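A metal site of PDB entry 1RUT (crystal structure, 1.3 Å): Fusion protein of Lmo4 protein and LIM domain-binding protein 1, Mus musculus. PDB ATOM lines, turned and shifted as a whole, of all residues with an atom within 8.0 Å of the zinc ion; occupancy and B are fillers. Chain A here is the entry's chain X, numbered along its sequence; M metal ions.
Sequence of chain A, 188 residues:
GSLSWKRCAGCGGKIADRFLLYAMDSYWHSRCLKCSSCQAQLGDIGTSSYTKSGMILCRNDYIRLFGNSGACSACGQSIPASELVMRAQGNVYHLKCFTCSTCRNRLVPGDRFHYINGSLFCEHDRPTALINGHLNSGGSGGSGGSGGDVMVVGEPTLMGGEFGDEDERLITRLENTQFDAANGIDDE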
ATOM      1  N   ARG A   7      -8.215  18.886   1.878  1.00  0.00           N
ATOM      2  CA  ARG A   7      -9.288  17.925   1.669  1.00  0.00           C
ATOM      3  C   ARG A   7      -8.681  16.627   1.184  1.00  0.00           C
ATOM      4  O   ARG A   7      -7.706  16.626   0.438  1.00  0.00           O
ATOM      5  CB  ARG A   7     -10.307  18.480   0.670  1.00  0.00           C
ATOM      6  CG  ARG A   7     -10.962  19.761   1.161  1.00  0.00           C
ATOM      7  CD  ARG A   7     -12.393  19.971   0.723  1.00  0.00           C
ATOM      8  NE  ARG A   7     -13.111  20.876   1.617  1.00  0.00           N
ATOM      9  CZ  ARG A   7     -14.125  20.529   2.415  1.00  0.00           C
ATOM     10  NH1 ARG A   7     -14.557  19.275   2.491  1.00  0.00           N
ATOM     11  NH2 ARG A   7     -14.703  21.460   3.177  1.00  0.00           N
ATOM     12  N   CYS A   8      -9.294  15.536   1.604  1.00  0.00           N
ATOM     13  CA  CYS A   8      -8.885  14.185   1.276  1.00  0.00           C
ATOM     14  C   CYS A   8      -9.441  13.775  -0.092  1.00  0.00           C
ATOM     15  O   CYS A   8     -10.648  13.910  -0.350  1.00  0.00           O
ATOM     16  CB  CYS A   8      -9.426  13.250   2.338  1.00  0.00           C
ATOM     17  SG  CYS A   8      -9.088  11.507   2.038  1.00  0.00           S
ATOM     18  N   ALA A   9      -8.580  13.280  -0.957  1.00  0.00           N
ATOM     19  CA  ALA A   9      -9.018  12.795  -2.269  1.00  0.00           C
ATOM     20  C   ALA A   9      -9.839  11.512  -2.192  1.00  0.00           C
ATOM     21  O   ALA A   9     -10.515  11.162  -3.135  1.00  0.00           O
ATOM     22  CB  ALA A   9      -7.816  12.601  -3.170  1.00  0.00           C
ATOM     23  N   GLY A  10      -9.755  10.800  -1.083  1.00  0.00           N
ATOM     24  CA  GLY A  10     -10.489   9.564  -0.908  1.00  0.00           C
ATOM     25  C   GLY A  10     -11.929   9.752  -0.456  1.00  0.00           C
ATOM     26  O   GLY A  10     -12.824   9.057  -0.950  1.00  0.00           O
ATOM     27  N   CYS A  11     -12.168  10.682   0.454  1.00  0.00           N
ATOM     28  CA  CYS A  11     -13.498  10.884   1.034  1.00  0.00           C
ATOM     29  C   CYS A  11     -14.073  12.282   0.844  1.00  0.00           C
ATOM     30  O   CYS A  11     -15.236  12.492   1.148  1.00  0.00           O
ATOM     31  CB  CYS A  11     -13.521  10.518   2.515  1.00  0.00           C
ATOM     32  SG  CYS A  11     -12.614  11.705   3.554  1.00  0.00           S
ATOM     33  N   GLY A  12     -13.267  13.223   0.368  1.00  0.00           N
ATOM     34  CA  GLY A  12     -13.716  14.608   0.202  1.00  0.00           C
ATOM     35  C   GLY A  12     -13.744  15.443   1.465  1.00  0.00           C
ATOM     36  O   GLY A  12     -14.023  16.637   1.389  1.00  0.00           O
ATOM     37  N   GLY A  13     -13.477  14.848   2.619  1.00  0.00           N
ATOM     38  CA  GLY A  13     -13.579  15.534   3.887  1.00  0.00           C
ATOM     39  C   GLY A  13     -12.308  16.282   4.229  1.00  0.00           C
ATOM     40  O   GLY A  13     -11.229  15.949   3.739  1.00  0.00           O
ATOM     41  N   LYS A  14     -12.419  17.289   5.078  1.00  0.00           N
ATOM     42  CA  LYS A  14     -11.260  17.989   5.587  1.00  0.00           C
ATOM     43  C   LYS A  14     -10.416  17.031   6.423  1.00  0.00           C
ATOM     44  O   LYS A  14     -10.939  16.161   7.127  1.00  0.00           O
ATOM     45  CB  LYS A  14     -11.675  19.218   6.391  1.00  0.00           C
ATOM     46  CG  LYS A  14     -12.347  20.290   5.525  1.00  0.00           C
ATOM     47  CD  LYS A  14     -12.348  21.684   6.152  1.00  0.00           C
ATOM     48  CE  LYS A  14     -13.526  21.889   7.088  1.00  0.00           C
ATOM     49  NZ  LYS A  14     -13.416  21.066   8.317  1.00  0.00           N
ATOM     50  N   ILE A  15      -9.095  17.214   6.353  1.00  0.00           N
ATOM     51  CA  ILE A  15      -8.177  16.362   7.096  1.00  0.00           C
ATOM     52  C   ILE A  15      -7.678  17.145   8.295  1.00  0.00           C
ATOM     53  O   ILE A  15      -6.809  18.012   8.193  1.00  0.00           O
ATOM     54  CB  ILE A  15      -6.995  15.900   6.222  1.00  0.00           C
ATOM     55  CG1 ILE A  15      -7.473  15.134   4.975  1.00  0.00           C
ATOM     56  CG2 ILE A  15      -6.092  14.990   7.041  1.00  0.00           C
ATOM     57  CD1 ILE A  15      -6.410  15.041   3.912  1.00  0.00           C
ATOM     58  N   ASP A  17      -6.539  15.376  10.941  1.00  0.00           N
ATOM     59  CA  ASP A  17      -5.654  14.409  11.593  1.00  0.00           C
ATOM     60  C   ASP A  17      -4.256  14.989  11.760  1.00  0.00           C
ATOM     61  O   ASP A  17      -3.775  15.713  10.903  1.00  0.00           O
ATOM     62  CB  ASP A  17      -5.500  13.152  10.744  1.00  0.00           C
ATOM     63  CG  ASP A  17      -6.770  12.381  10.573  1.00  0.00           C
ATOM     64  OD1 ASP A  17      -7.873  12.768  11.040  1.00  0.00           O
ATOM     65  OD2 ASP A  17      -6.725  11.317   9.919  1.00  0.00           O
ATOM     66  N   TYR A  27      -3.783  15.044  -1.026  1.00  0.00           N
ATOM     67  CA  TYR A  27      -3.732  14.726   0.396  1.00  0.00           C
ATOM     68  C   TYR A  27      -4.764  13.672   0.715  1.00  0.00           C
ATOM     69  O   TYR A  27      -5.816  13.615   0.091  1.00  0.00           O
ATOM     70  CB  TYR A  27      -4.002  15.972   1.234  1.00  0.00           C
ATOM     71  CG  TYR A  27      -2.967  17.033   1.034  1.00  0.00           C
ATOM     72  CD1 TYR A  27      -3.109  17.994   0.042  1.00  0.00           C
ATOM     73  CD2 TYR A  27      -1.822  17.083   1.821  1.00  0.00           C
ATOM     74  CE1 TYR A  27      -2.158  18.972  -0.151  1.00  0.00           C
ATOM     75  CE2 TYR A  27      -0.879  18.072   1.653  1.00  0.00           C
ATOM     76  CZ  TYR A  27      -1.056  19.012   0.665  1.00  0.00           C
ATOM     77  OH  TYR A  27      -0.114  20.004   0.487  1.00  0.00           O
ATOM     78  N   TRP A  28      -4.484  12.877   1.748  1.00  0.00           N
ATOM     79  CA  TRP A  28      -5.348  11.780   2.142  1.00  0.00           C
ATOM     80  C   TRP A  28      -5.341  11.601   3.643  1.00  0.00           C
ATOM     81  O   TRP A  28      -4.285  11.653   4.254  1.00  0.00           O
ATOM     82  CB  TRP A  28      -4.838  10.455   1.556  1.00  0.00           C
ATOM     83  CG  TRP A  28      -4.569  10.469   0.097  1.00  0.00           C
ATOM     84  CD1 TRP A  28      -3.489  11.002  -0.525  1.00  0.00           C
ATOM     85  CD2 TRP A  28      -5.384   9.900  -0.938  1.00  0.00           C
ATOM     86  NE1 TRP A  28      -3.587  10.821  -1.881  1.00  0.00           N
ATOM     87  CE2 TRP A  28      -4.736  10.127  -2.156  1.00  0.00           C
ATOM     88  CE3 TRP A  28      -6.593   9.186  -0.943  1.00  0.00           C
ATOM     89  CZ2 TRP A  28      -5.258   9.702  -3.393  1.00  0.00           C
ATOM     90  CZ3 TRP A  28      -7.106   8.758  -2.160  1.00  0.00           C
ATOM     91  CH2 TRP A  28      -6.444   9.024  -3.366  1.00  0.00           C
ATOM     92  N   HIS A  29      -6.491  11.311   4.243  1.00  0.00           N
ATOM     93  CA  HIS A  29      -6.470  10.571   5.503  1.00  0.00           C
ATOM     94  C   HIS A  29      -5.810   9.232   5.182  1.00  0.00           C
ATOM     95  O   HIS A  29      -6.106   8.632   4.144  1.00  0.00           O
ATOM     96  CB  HIS A  29      -7.868  10.223   5.995  1.00  0.00           C
ATOM     97  CG  HIS A  29      -8.777  11.385   6.305  1.00  0.00           C
ATOM     98  ND1 HIS A  29      -9.813  11.767   5.470  1.00  0.00           N
ATOM     99  CD2 HIS A  29      -8.836  12.197   7.382  1.00  0.00           C
ATOM    100  CE1 HIS A  29     -10.450  12.784   6.031  1.00  0.00           C
ATOM    101  NE2 HIS A  29      -9.879  13.063   7.185  1.00  0.00           N
ATOM    102  N   SER A  30      -4.947   8.712   6.049  1.00  0.00           N
ATOM    103  CA  SER A  30      -4.310   7.446   5.722  1.00  0.00           C
ATOM    104  C   SER A  30      -5.334   6.335   5.440  1.00  0.00           C
ATOM    105  O   SER A  30      -5.196   5.556   4.488  1.00  0.00           O
ATOM    106  CB  SER A  30      -3.335   7.002   6.812  1.00  0.00           C
ATOM    107  OG  SER A  30      -2.701   5.811   6.404  1.00  0.00           O
ATOM    108  N   ARG A  31      -6.378   6.276   6.252  1.00  0.00           N
ATOM    109  CA  ARG A  31      -7.418   5.261   6.077  1.00  0.00           C
ATOM    110  C   ARG A  31      -8.123   5.332   4.737  1.00  0.00           C
ATOM    111  O   ARG A  31      -8.748   4.358   4.332  1.00  0.00           O
ATOM    112  CB  ARG A  31      -8.471   5.363   7.196  1.00  0.00           C
ATOM    113  CG  ARG A  31      -9.155   6.727   7.272  1.00  0.00           C
ATOM    114  CD  ARG A  31     -10.067   6.909   8.477  1.00  0.00           C
ATOM    115  NE  ARG A  31     -10.432   8.328   8.648  1.00  0.00           N
ATOM    116  CZ  ARG A  31     -11.416   8.942   8.006  1.00  0.00           C
ATOM    117  NH1 ARG A  31     -12.225   8.278   7.182  1.00  0.00           N
ATOM    118  NH2 ARG A  31     -11.621  10.224   8.232  1.00  0.00           N
ATOM    119  N   CYS A  32      -8.031   6.461   4.059  1.00  0.00           N
ATOM    120  CA  CYS A  32      -8.704   6.682   2.780  1.00  0.00           C
ATOM    121  C   CYS A  32      -7.870   6.321   1.559  1.00  0.00           C
ATOM    122  O   CYS A  32      -8.402   6.315   0.464  1.00  0.00           O
ATOM    123  CB  CYS A  32      -9.164   8.116   2.695  1.00  0.00           C
ATOM    124  SG  CYS A  32     -10.441   8.488   3.921  1.00  0.00           S
ATOM    125  N   LEU A  33      -6.570   6.061   1.741  1.00  0.00           N
ATOM    126  CA  LEU A  33      -5.702   5.666   0.635  1.00  0.00           C
ATOM    127  C   LEU A  33      -5.487   4.160   0.724  1.00  0.00           C
ATOM    128  O   LEU A  33      -4.680   3.667   1.496  1.00  0.00           O
ATOM    129  CB  LEU A  33      -4.377   6.433   0.666  1.00  0.00           C
ATOM    130  CG  LEU A  33      -3.421   6.074  -0.474  1.00  0.00           C
ATOM    131  CD1 LEU A  33      -4.047   6.291  -1.840  1.00  0.00           C
ATOM    132  CD2 LEU A  33      -2.133   6.867  -0.338  1.00  0.00           C
HETATM  133 ZN    ZN M   1     -10.501  10.777   3.764  1.00  0.00          ZN
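The guanidinium group of Arg 31 is in hydrogen-bond range of a ring nitrogen (NE2) of His 29 (3.5 Å). A ring nitrogen (NE2) of His 29 is in hydrogen-bond range of the backbone carbonyl oxygen (O) of Lys 14 (3.3 Å). SG of Cys 32 sits close to NH1 of Arg 31. N of Gly 13 lies close to SG of Cys 11. The side-chain sulfur (SG) of Cys 8 lies close to the backbone NH (N) of Gly 10, 3.3 Å away. The backbone carbonyl oxygen of Gly 13 sits at hydrogen-bond distance from the backbone NH of Cys 8 (2.9 Å).
ND1 of His 29 is bound to the zinc ion. The zinc ion is bound by SG of Cys 32 (2.3 Å). SG of Cys 11 binds the zinc ion (2.3 Å). The side-chain sulfur (SG) of Cys 8 is bound to the zinc ion, at 2.3 Å.
Within 4 Å of the zinc ion: Cys 8, Cys 11, His 29 and Cys 32.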
